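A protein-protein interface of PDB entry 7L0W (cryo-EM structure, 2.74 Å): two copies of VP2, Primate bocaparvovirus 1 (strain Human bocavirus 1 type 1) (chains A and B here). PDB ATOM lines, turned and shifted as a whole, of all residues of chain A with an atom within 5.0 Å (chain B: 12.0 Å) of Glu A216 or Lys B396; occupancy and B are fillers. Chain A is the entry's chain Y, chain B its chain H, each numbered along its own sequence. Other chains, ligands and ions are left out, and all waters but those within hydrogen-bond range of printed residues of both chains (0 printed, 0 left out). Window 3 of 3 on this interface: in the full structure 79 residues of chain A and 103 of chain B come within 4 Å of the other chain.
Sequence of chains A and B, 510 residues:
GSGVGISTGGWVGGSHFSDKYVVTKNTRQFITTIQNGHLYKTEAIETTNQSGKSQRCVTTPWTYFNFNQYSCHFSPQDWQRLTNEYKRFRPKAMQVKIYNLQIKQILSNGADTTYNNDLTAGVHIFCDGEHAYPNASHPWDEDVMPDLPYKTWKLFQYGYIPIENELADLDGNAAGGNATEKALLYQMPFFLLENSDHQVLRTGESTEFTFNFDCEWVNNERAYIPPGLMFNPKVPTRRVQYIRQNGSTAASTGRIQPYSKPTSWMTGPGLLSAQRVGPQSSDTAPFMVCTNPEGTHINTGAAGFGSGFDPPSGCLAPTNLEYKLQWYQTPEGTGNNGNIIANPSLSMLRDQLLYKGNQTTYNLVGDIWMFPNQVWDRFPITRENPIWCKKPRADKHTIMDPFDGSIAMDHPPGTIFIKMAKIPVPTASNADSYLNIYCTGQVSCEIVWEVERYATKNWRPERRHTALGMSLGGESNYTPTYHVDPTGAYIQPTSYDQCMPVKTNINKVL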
ATOM      1  N   PHE A  89     -26.281  24.547   4.299  1.00  0.00           N
ATOM      2  CA  PHE A  89     -26.012  25.396   3.151  1.00  0.00           C
ATOM      3  C   PHE A  89     -25.789  24.543   1.913  1.00  0.00           C
ATOM      4  O   PHE A  89     -25.263  23.434   1.995  1.00  0.00           O
ATOM      5  CB  PHE A  89     -24.803  26.289   3.411  1.00  0.00           C
ATOM      6  CG  PHE A  89     -23.562  25.536   3.764  1.00  0.00           C
ATOM      7  CD1 PHE A  89     -22.672  25.147   2.789  1.00  0.00           C
ATOM      8  CD2 PHE A  89     -23.286  25.215   5.077  1.00  0.00           C
ATOM      9  CE1 PHE A  89     -21.537  24.462   3.115  1.00  0.00           C
ATOM     10  CE2 PHE A  89     -22.153  24.527   5.402  1.00  0.00           C
ATOM     11  CZ  PHE A  89     -21.277  24.149   4.419  1.00  0.00           C
ATOM     12  N   ARG A  90     -26.187  25.073   0.759  1.00  0.00           N
ATOM     13  CA  ARG A  90     -25.885  24.428  -0.513  1.00  0.00           C
ATOM     14  C   ARG A  90     -25.708  25.503  -1.578  1.00  0.00           C
ATOM     15  O   ARG A  90     -26.192  26.627  -1.415  1.00  0.00           O
ATOM     16  CB  ARG A  90     -26.983  23.437  -0.919  1.00  0.00           C
ATOM     17  CG  ARG A  90     -28.301  24.073  -1.166  1.00  0.00           C
ATOM     18  CD  ARG A  90     -29.278  23.068  -1.674  1.00  0.00           C
ATOM     19  NE  ARG A  90     -30.578  23.678  -1.883  1.00  0.00           N
ATOM     20  CZ  ARG A  90     -31.649  23.005  -2.269  1.00  0.00           C
ATOM     21  NH1 ARG A  90     -31.560  21.703  -2.487  1.00  0.00           N
ATOM     22  NH2 ARG A  90     -32.802  23.632  -2.434  1.00  0.00           N
ATOM     23  N   ASP A 214     -28.503  21.769  -8.625  1.00  0.00           N
ATOM     24  CA  ASP A 214     -29.546  21.237  -7.754  1.00  0.00           C
ATOM     25  C   ASP A 214     -28.903  20.030  -7.066  1.00  0.00           C
ATOM     26  O   ASP A 214     -28.492  19.082  -7.731  1.00  0.00           O
ATOM     27  CB  ASP A 214     -30.800  20.865  -8.509  1.00  0.00           C
ATOM     28  CG  ASP A 214     -31.955  20.557  -7.587  1.00  0.00           C
ATOM     29  OD1 ASP A 214     -31.784  20.696  -6.357  1.00  0.00           O
ATOM     30  OD2 ASP A 214     -33.034  20.193  -8.094  1.00  0.00           O
ATOM     31  N   CYS A 215     -28.806  20.093  -5.740  1.00  0.00           N
ATOM     32  CA  CYS A 215     -28.044  19.097  -5.005  1.00  0.00           C
ATOM     33  C   CYS A 215     -28.512  19.061  -3.558  1.00  0.00           C
ATOM     34  O   CYS A 215     -29.394  19.820  -3.145  1.00  0.00           O
ATOM     35  CB  CYS A 215     -26.542  19.382  -5.093  1.00  0.00           C
ATOM     36  SG  CYS A 215     -26.057  21.029  -4.546  1.00  0.00           S
ATOM     37  N   GLU A 216     -27.914  18.158  -2.792  1.00  0.00           N
ATOM     38  CA  GLU A 216     -28.279  17.975  -1.400  1.00  0.00           C
ATOM     39  C   GLU A 216     -27.609  19.014  -0.512  1.00  0.00           C
ATOM     40  O   GLU A 216     -26.575  19.588  -0.854  1.00  0.00           O
ATOM     41  CB  GLU A 216     -27.903  16.576  -0.928  1.00  0.00           C
ATOM     42  CG  GLU A 216     -26.426  16.282  -1.022  1.00  0.00           C
ATOM     43  CD  GLU A 216     -26.103  14.873  -0.590  1.00  0.00           C
ATOM     44  OE1 GLU A 216     -26.934  14.277   0.121  1.00  0.00           O
ATOM     45  OE2 GLU A 216     -25.032  14.354  -0.973  1.00  0.00           O
ATOM     46  N   TRP A 217     -28.220  19.245   0.644  1.00  0.00           N
ATOM     47  CA  TRP A 217     -27.714  20.193   1.617  1.00  0.00           C
ATOM     48  C   TRP A 217     -26.468  19.656   2.308  1.00  0.00           C
ATOM     49  O   TRP A 217     -26.182  18.459   2.293  1.00  0.00           O
ATOM     50  CB  TRP A 217     -28.781  20.492   2.658  1.00  0.00           C
ATOM     51  CG  TRP A 217     -29.932  21.228   2.125  1.00  0.00           C
ATOM     52  CD1 TRP A 217     -31.053  20.700   1.582  1.00  0.00           C
ATOM     53  CD2 TRP A 217     -30.109  22.641   2.113  1.00  0.00           C
ATOM     54  NE1 TRP A 217     -31.915  21.694   1.212  1.00  0.00           N
ATOM     55  CE2 TRP A 217     -31.355  22.900   1.533  1.00  0.00           C
ATOM     56  CE3 TRP A 217     -29.331  23.716   2.530  1.00  0.00           C
ATOM     57  CZ2 TRP A 217     -31.838  24.185   1.361  1.00  0.00           C
ATOM     58  CZ3 TRP A 217     -29.814  24.982   2.362  1.00  0.00           C
ATOM     59  CH2 TRP A 217     -31.051  25.210   1.785  1.00  0.00           C
ATOM     60  N   VAL A 218     -25.717  20.566   2.914  1.00  0.00           N
ATOM     61  CA  VAL A 218     -24.608  20.222   3.792  1.00  0.00           C
ATOM     62  C   VAL A 218     -24.991  20.658   5.196  1.00  0.00           C
ATOM     63  O   VAL A 218     -25.063  21.856   5.480  1.00  0.00           O
ATOM     64  CB  VAL A 218     -23.300  20.883   3.350  1.00  0.00           C
ATOM     65  CG1 VAL A 218     -22.210  20.562   4.329  1.00  0.00           C
ATOM     66  CG2 VAL A 218     -22.920  20.410   1.980  1.00  0.00           C
ATOM     67  N   GLN A 374     -30.200   1.990   9.527  1.00  0.00           N
ATOM     68  CA  GLN A 374     -28.906   2.618   9.742  1.00  0.00           C
ATOM     69  C   GLN A 374     -29.035   4.112   9.521  1.00  0.00           C
ATOM     70  O   GLN A 374     -29.560   4.546   8.496  1.00  0.00           O
ATOM     71  CB  GLN A 374     -27.842   2.035   8.821  1.00  0.00           C
ATOM     72  CG  GLN A 374     -27.403   0.659   9.205  1.00  0.00           C
ATOM     73  CD  GLN A 374     -26.346   0.150   8.283  1.00  0.00           C
ATOM     74  OE1 GLN A 374     -26.278   0.557   7.133  1.00  0.00           O
ATOM     75  NE2 GLN A 374     -25.490  -0.720   8.785  1.00  0.00           N
ATOM     76  N   VAL A 375     -28.569   4.891  10.491  1.00  0.00           N
ATOM     77  CA  VAL A 375     -28.588   6.344  10.425  1.00  0.00           C
ATOM     78  C   VAL A 375     -27.189   6.846  10.735  1.00  0.00           C
ATOM     79  O   VAL A 375     -26.542   6.357  11.666  1.00  0.00           O
ATOM     80  CB  VAL A 375     -29.620   6.947  11.393  1.00  0.00           C
ATOM     81  CG1 VAL A 375     -31.010   6.591  10.952  1.00  0.00           C
ATOM     82  CG2 VAL A 375     -29.398   6.431  12.789  1.00  0.00           C
ATOM     83  N   TRP A 376     -26.715   7.800   9.943  1.00  0.00           N
ATOM     84  CA  TRP A 376     -25.387   8.341  10.162  1.00  0.00           C
ATOM     85  C   TRP A 376     -25.304   9.724   9.545  1.00  0.00           C
ATOM     86  O   TRP A 376     -26.154  10.122   8.748  1.00  0.00           O
ATOM     87  CB  TRP A 376     -24.307   7.429   9.585  1.00  0.00           C
ATOM     88  CG  TRP A 376     -24.260   7.317   8.098  1.00  0.00           C
ATOM     89  CD1 TRP A 376     -23.484   8.044   7.257  1.00  0.00           C
ATOM     90  CD2 TRP A 376     -24.990   6.406   7.278  1.00  0.00           C
ATOM     91  NE1 TRP A 376     -23.690   7.655   5.964  1.00  0.00           N
ATOM     92  CE2 TRP A 376     -24.613   6.646   5.951  1.00  0.00           C
ATOM     93  CE3 TRP A 376     -25.933   5.415   7.537  1.00  0.00           C
ATOM     94  CZ2 TRP A 376     -25.142   5.934   4.887  1.00  0.00           C
ATOM     95  CZ3 TRP A 376     -26.456   4.714   6.482  1.00  0.00           C
ATOM     96  CH2 TRP A 376     -26.061   4.973   5.175  1.00  0.00           C
ATOM     97  N   ARG A 378     -22.817  12.478   7.398  1.00  0.00           N
ATOM     98  CA  ARG A 378     -21.732  12.535   6.445  1.00  0.00           C
ATOM     99  C   ARG A 378     -20.501  13.151   7.088  1.00  0.00           C
ATOM    100  O   ARG A 378     -20.568  13.756   8.157  1.00  0.00           O
ATOM    101  CB  ARG A 378     -22.137  13.337   5.222  1.00  0.00           C
ATOM    102  CG  ARG A 378     -23.350  12.806   4.536  1.00  0.00           C
ATOM    103  CD  ARG A 378     -23.518  13.532   3.256  1.00  0.00           C
ATOM    104  NE  ARG A 378     -22.368  13.250   2.412  1.00  0.00           N
ATOM    105  CZ  ARG A 378     -22.143  13.831   1.247  1.00  0.00           C
ATOM    106  NH1 ARG A 378     -22.989  14.735   0.782  1.00  0.00           N
ATOM    107  NH2 ARG A 378     -21.070  13.512   0.551  1.00  0.00           N
ATOM    108  N   ILE A 399     -27.068   4.153  -1.999  1.00  0.00           N
ATOM    109  CA  ILE A 399     -27.066   5.488  -1.422  1.00  0.00           C
ATOM    110  C   ILE A 399     -25.712   6.135  -1.662  1.00  0.00           C
ATOM    111  O   ILE A 399     -24.670   5.478  -1.580  1.00  0.00           O
ATOM    112  CB  ILE A 399     -27.412   5.406   0.071  1.00  0.00           C
ATOM    113  CG1 ILE A 399     -27.488   6.792   0.700  1.00  0.00           C
ATOM    114  CG2 ILE A 399     -26.414   4.561   0.803  1.00  0.00           C
ATOM    115  CD1 ILE A 399     -28.095   6.780   2.072  1.00  0.00           C
ATOM    116  N   MET A 400     -25.718   7.434  -1.963  1.00  0.00           N
ATOM    117  CA  MET A 400     -24.488   8.153  -2.282  1.00  0.00           C
ATOM    118  C   MET A 400     -24.065   8.928  -1.041  1.00  0.00           C
ATOM    119  O   MET A 400     -24.579  10.001  -0.741  1.00  0.00           O
ATOM    120  CB  MET A 400     -24.723   9.106  -3.448  1.00  0.00           C
ATOM    121  CG  MET A 400     -25.134   8.489  -4.765  1.00  0.00           C
ATOM    122  SD  MET A 400     -23.813   7.690  -5.673  1.00  0.00           S
ATOM    123  CE  MET A 400     -24.071   5.982  -5.245  1.00  0.00           C
ATOM    124  N   ASP A 401     -23.110   8.375  -0.312  1.00  0.00           N
ATOM    125  CA  ASP A 401     -22.302   9.153   0.621  1.00  0.00           C
ATOM    126  C   ASP A 401     -20.839   8.952   0.289  1.00  0.00           C
ATOM    127  O   ASP A 401     -20.281   7.889   0.618  1.00  0.00           O
ATOM    128  CB  ASP A 401     -22.576   8.753   2.067  1.00  0.00           C
ATOM    129  CG  ASP A 401     -21.682   9.477   3.043  1.00  0.00           C
ATOM    130  OD1 ASP A 401     -21.673  10.722   3.024  1.00  0.00           O
ATOM    131  OD2 ASP A 401     -20.993   8.805   3.842  1.00  0.00           O
ATOM    132  N   ILE A 407     -20.042  16.096  -2.228  1.00  0.00           N
ATOM    133  CA  ILE A 407     -21.377  15.827  -2.744  1.00  0.00           C
ATOM    134  C   ILE A 407     -21.257  15.168  -4.106  1.00  0.00           C
ATOM    135  O   ILE A 407     -20.562  15.671  -4.992  1.00  0.00           O
ATOM    136  CB  ILE A 407     -22.194  17.120  -2.837  1.00  0.00           C
ATOM    137  CG1 ILE A 407     -22.434  17.704  -1.455  1.00  0.00           C
ATOM    138  CG2 ILE A 407     -23.513  16.858  -3.516  1.00  0.00           C
ATOM    139  CD1 ILE A 407     -23.028  19.077  -1.501  1.00  0.00           C
ATOM    140  N   ALA A 408     -21.952  14.058  -4.292  1.00  0.00           N
ATOM    141  CA  ALA A 408     -21.933  13.350  -5.561  1.00  0.00           C
ATOM    142  C   ALA A 408     -23.038  13.907  -6.440  1.00  0.00           C
ATOM    143  O   ALA A 408     -24.222  13.726  -6.147  1.00  0.00           O
ATOM    144  CB  ALA A 408     -22.115  11.850  -5.356  1.00  0.00           C
ATOM    145  N   MET B 370     -28.081  -5.793   3.755  1.00  0.00           N
ATOM    146  CA  MET B 370     -28.825  -5.355   2.583  1.00  0.00           C
ATOM    147  C   MET B 370     -28.085  -5.781   1.335  1.00  0.00           C
ATOM    148  O   MET B 370     -26.866  -5.632   1.235  1.00  0.00           O
ATOM    149  CB  MET B 370     -29.057  -3.848   2.582  1.00  0.00           C
ATOM    150  CG  MET B 370     -30.168  -3.393   3.498  1.00  0.00           C
ATOM    151  SD  MET B 370     -30.332  -1.604   3.591  1.00  0.00           S
ATOM    152  CE  MET B 370     -30.926  -1.221   1.959  1.00  0.00           C
ATOM    153  N   LYS B 390     -39.930   7.481  16.305  1.00  0.00           N
ATOM    154  CA  LYS B 390     -39.396   8.735  15.804  1.00  0.00           C
ATOM    155  C   LYS B 390     -38.102   8.474  15.054  1.00  0.00           C
ATOM    156  O   LYS B 390     -37.122   8.007  15.639  1.00  0.00           O
ATOM    157  CB  LYS B 390     -39.162   9.750  16.916  1.00  0.00           C
ATOM    158  CG  LYS B 390     -38.670  11.050  16.353  1.00  0.00           C
ATOM    159  CD  LYS B 390     -38.484  12.103  17.393  1.00  0.00           C
ATOM    160  CE  LYS B 390     -37.780  13.290  16.778  1.00  0.00           C
ATOM    161  NZ  LYS B 390     -38.559  13.843  15.645  1.00  0.00           N
ATOM    162  N   LYS B 391     -38.103   8.781  13.769  1.00  0.00           N
ATOM    163  CA  LYS B 391     -36.911   8.630  12.958  1.00  0.00           C
ATOM    164  C   LYS B 391     -35.903   9.713  13.323  1.00  0.00           C
ATOM    165  O   LYS B 391     -36.258  10.892  13.390  1.00  0.00           O
ATOM    166  CB  LYS B 391     -37.270   8.738  11.482  1.00  0.00           C
ATOM    167  CG  LYS B 391     -36.141   8.453  10.535  1.00  0.00           C
ATOM    168  CD  LYS B 391     -36.547   8.821   9.130  1.00  0.00           C
ATOM    169  CE  LYS B 391     -37.673   7.939   8.651  1.00  0.00           C
ATOM    170  NZ  LYS B 391     -38.114   8.304   7.284  1.00  0.00           N
ATOM    171  N   PRO B 392     -34.647   9.351  13.564  1.00  0.00           N
ATOM    172  CA  PRO B 392     -33.647  10.364  13.899  1.00  0.00           C
ATOM    173  C   PRO B 392     -33.430  11.339  12.755  1.00  0.00           C
ATOM    174  O   PRO B 392     -33.692  11.039  11.590  1.00  0.00           O
ATOM    175  CB  PRO B 392     -32.389   9.536  14.158  1.00  0.00           C
ATOM    176  CG  PRO B 392     -32.891   8.214  14.518  1.00  0.00           C
ATOM    177  CD  PRO B 392     -34.099   7.998  13.677  1.00  0.00           C
ATOM    178  N   ARG B 393     -32.929  12.515  13.103  1.00  0.00           N
ATOM    179  CA  ARG B 393     -32.572  13.523  12.112  1.00  0.00           C
ATOM    180  C   ARG B 393     -31.114  13.287  11.772  1.00  0.00           C
ATOM    181  O   ARG B 393     -30.230  13.500  12.601  1.00  0.00           O
ATOM    182  CB  ARG B 393     -32.804  14.923  12.659  1.00  0.00           C
ATOM    183  CG  ARG B 393     -34.252  15.216  12.938  1.00  0.00           C
ATOM    184  CD  ARG B 393     -34.445  16.571  13.560  1.00  0.00           C
ATOM    185  NE  ARG B 393     -35.850  16.807  13.863  1.00  0.00           N
ATOM    186  CZ  ARG B 393     -36.306  17.863  14.523  1.00  0.00           C
ATOM    187  NH1 ARG B 393     -35.467  18.788  14.961  1.00  0.00           N
ATOM    188  NH2 ARG B 393     -37.605  17.991  14.747  1.00  0.00           N
ATOM    189  N   ALA B 394     -30.863  12.837  10.554  1.00  0.00           N
ATOM    190  CA  ALA B 394     -29.533  12.450  10.130  1.00  0.00           C
ATOM    191  C   ALA B 394     -29.412  12.655   8.632  1.00  0.00           C
ATOM    192  O   ALA B 394     -30.404  12.610   7.903  1.00  0.00           O
ATOM    193  CB  ALA B 394     -29.241  11.000  10.483  1.00  0.00           C
ATOM    194  N   ASP B 395     -28.182  12.880   8.179  1.00  0.00           N
ATOM    195  CA  ASP B 395     -27.964  13.141   6.767  1.00  0.00           C
ATOM    196  C   ASP B 395     -28.395  11.960   5.920  1.00  0.00           C
ATOM    197  O   ASP B 395     -29.248  12.095   5.036  1.00  0.00           O
ATOM    198  CB  ASP B 395     -26.495  13.450   6.519  1.00  0.00           C
ATOM    199  CG  ASP B 395     -26.047  14.684   7.235  1.00  0.00           C
ATOM    200  OD1 ASP B 395     -26.915  15.426   7.725  1.00  0.00           O
ATOM    201  OD2 ASP B 395     -24.830  14.918   7.309  1.00  0.00           O
ATOM    202  N   LYS B 396     -27.825  10.793   6.183  1.00  0.00           N
ATOM    203  CA  LYS B 396     -28.081   9.600   5.400  1.00  0.00           C
ATOM    204  C   LYS B 396     -28.771   8.567   6.269  1.00  0.00           C
ATOM    205  O   LYS B 396     -28.538   8.508   7.477  1.00  0.00           O
ATOM    206  CB  LYS B 396     -26.785   9.029   4.847  1.00  0.00           C
ATOM    207  CG  LYS B 396     -25.999   9.992   4.001  1.00  0.00           C
ATOM    208  CD  LYS B 396     -26.764  10.381   2.762  1.00  0.00           C
ATOM    209  CE  LYS B 396     -25.955  11.324   1.902  1.00  0.00           C
ATOM    210  NZ  LYS B 396     -26.691  11.725   0.681  1.00  0.00           N
ATOM    211  N   HIS B 397     -29.638   7.774   5.654  1.00  0.00           N
ATOM    212  CA  HIS B 397     -30.222   6.627   6.327  1.00  0.00           C
ATOM    213  C   HIS B 397     -30.627   5.610   5.278  1.00  0.00           C
ATOM    214  O   HIS B 397     -30.942   5.970   4.144  1.00  0.00           O
ATOM    215  CB  HIS B 397     -31.420   7.029   7.183  1.00  0.00           C
ATOM    216  CG  HIS B 397     -32.546   7.626   6.404  1.00  0.00           C
ATOM    217  ND1 HIS B 397     -33.446   6.864   5.695  1.00  0.00           N
ATOM    218  CD2 HIS B 397     -32.919   8.913   6.223  1.00  0.00           C
ATOM    219  CE1 HIS B 397     -34.328   7.654   5.113  1.00  0.00           C
ATOM    220  NE2 HIS B 397     -34.028   8.905   5.416  1.00  0.00           N
ATOM    221  N   THR B 398     -30.626   4.343   5.669  1.00  0.00           N
ATOM    222  CA  THR B 398     -31.015   3.265   4.777  1.00  0.00           C
ATOM    223  C   THR B 398     -32.533   3.108   4.810  1.00  0.00           C
ATOM    224  O   THR B 398     -33.260   3.988   5.268  1.00  0.00           O
ATOM    225  CB  THR B 398     -30.317   1.966   5.153  1.00  0.00           C
ATOM    226  OG1 THR B 398     -30.709   1.588   6.471  1.00  0.00           O
ATOM    227  CG2 THR B 398     -28.830   2.142   5.115  1.00  0.00           C
ATOM    228  N   ILE B 399     -33.025   1.997   4.267  1.00  0.00           N
ATOM    229  CA  ILE B 399     -34.446   1.694   4.336  1.00  0.00           C
ATOM    230  C   ILE B 399     -34.867   1.603   5.794  1.00  0.00           C
ATOM    231  O   ILE B 399     -34.130   1.080   6.637  1.00  0.00           O
ATOM    232  CB  ILE B 399     -34.736   0.399   3.567  1.00  0.00           C
ATOM    233  CG1 ILE B 399     -36.225   0.081   3.559  1.00  0.00           C
ATOM    234  CG2 ILE B 399     -33.967  -0.749   4.149  1.00  0.00           C
ATOM    235  CD1 ILE B 399     -36.587  -1.007   2.590  1.00  0.00           C
ATOM    236  N   MET B 400     -36.059   2.114   6.103  1.00  0.00           N
ATOM    237  CA  MET B 400     -36.545   2.147   7.480  1.00  0.00           C
ATOM    238  C   MET B 400     -37.523   0.994   7.656  1.00  0.00           C
ATOM    239  O   MET B 400     -38.686   1.067   7.275  1.00  0.00           O
ATOM    240  CB  MET B 400     -37.236   3.478   7.761  1.00  0.00           C
ATOM    241  CG  MET B 400     -36.392   4.726   7.645  1.00  0.00           C
ATOM    242  SD  MET B 400     -35.269   5.011   9.008  1.00  0.00           S
ATOM    243  CE  MET B 400     -33.738   4.394   8.344  1.00  0.00           C
ATOM    244  N   ALA B 408     -41.531   4.258  11.481  1.00  0.00           N
ATOM    245  CA  ALA B 408     -40.562   5.309  11.739  1.00  0.00           C
ATOM    246  C   ALA B 408     -41.033   6.577  11.050  1.00  0.00           C
ATOM    247  O   ALA B 408     -41.055   6.648   9.818  1.00  0.00           O
ATOM    248  CB  ALA B 408     -39.176   4.911  11.245  1.00  0.00           C
ATOM    249  N   ASP B 410     -40.562  10.819  10.807  1.00  0.00           N
ATOM    250  CA  ASP B 410     -39.620  11.881  11.130  1.00  0.00           C
ATOM    251  C   ASP B 410     -40.314  13.021  11.857  1.00  0.00           C
ATOM    252  O   ASP B 410     -39.658  13.907  12.411  1.00  0.00           O
ATOM    253  CB  ASP B 410     -38.930  12.369   9.862  1.00  0.00           C
ATOM    254  CG  ASP B 410     -39.903  12.819   8.819  1.00  0.00           C
ATOM    255  OD1 ASP B 410     -41.118  12.649   9.040  1.00  0.00           O
ATOM    256  OD2 ASP B 410     -39.456  13.332   7.774  1.00  0.00           O
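Among the printed residues, merely in contact across the chains: Gln A374 with His B397 (3.1 Å), Val A375 with Lys B396 (3.7 Å), Val A375 with His B397 (3.8 Å), Trp A376 with Ala B394 (3.6 Å), Trp A376 with Thr B398 (3.8 Å), Arg A378 with Lys B396 (3.6 Å), Ile A399 with Lys B396 (3.8 Å) and Ile A399 with His B397 (3.6 Å).
Arg A90 touches none of the printed residues of chain B.
No residue of chain B comes within 4 Å of Asp A214.
No residue of chain B comes within 4 Å of Cys A215.
Glu A216 touches just one residue of chain B: Lys B396.
No residue of chain B comes within 4 Å of Val A218.
Of the printed residues of chain B, Gln A374 touches His B397 (3.1 Å) and Thr B398 (3.0 Å).
Of chain B, only Lys B396 (3.7 Å) and His B397 (3.8 Å) come within 4 Å of Val A375.
Of chain B, only Ala B394 (3.6 Å), Asp B395 (3.5 Å), Lys B396 (3.1 Å) and Thr B398 (3.8 Å) come within 4 Å of Trp A376.
Of the printed residues of chain B, Arg A378 touches Asp B395 (3.2 Å) and Lys B396 (3.6 Å).
No residue of chain B comes within 4 Å of Asp A401.
No residue of chain B comes within 4 Å of Ile A407.
Pro B392 touches none of the printed residues of chain A.
Of the printed residues of chain A, Ala B394 touches Trp A376.
Printed residues of chain A within 4 Å of Asp B395: Trp A376 and Arg A378.
The nearest residue of chain B that does not touch Glu A216 is Asp B395 (5.9 Å).
The nearest printed residue of chain A that does not touch His B397 is Trp A376 (4.2 Å).
Of the 14 printed residues of chain B, 5 touch a printed residue of chain A.
Hydrophobic or aromatic side chains of chain B within 4 Å of the printed part of chain A: Ala B394 and His B397.
Along chain A the printed residues that touch a printed residue of chain B span positions 216 to 400.
Among the printed residues, 14 pairs touch across the chains.
Among the printed residues, Asp or Glu carboxylates within 4 Å of a Lys or Arg side-chain nitrogen of the other chain: Glu A216 with Lys B396.
N of Asp B395 lies within hydrogen-bond range of O of Trp A376 (3.5 Å).
The side-chain carboxylate of Asp B395 lies within hydrogen-bond range of the backbone NH of Arg A378 (3.2 Å).
OE1 of Glu A216 lies within salt-bridge range of NZ of Lys B396 (2.6 Å).
The backbone NH (N) of Lys B396 is in hydrogen-bond range of the backbone carbonyl oxygen (O) of Trp A376, at 3.1 Å.
The backbone carbonyl oxygen (O) of Met A400 lies within hydrogen-bond range of the side-chain amino group (NZ) of Lys B396.
The backbone NH (N) of Thr B398 is in hydrogen-bond range of the backbone carbonyl oxygen (O) of Gln A374 (3.0 Å).
The side-chain carboxylate (OE2) of Glu A216 is in salt-bridge range of the guanidinium group (NH1) of Arg A378.
The guanidinium group (NE) of Arg A378 lies within salt-bridge range of the side-chain carboxylate (OD1) of Asp A401 (2.7 Å).
3 positions are printed for both chains.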
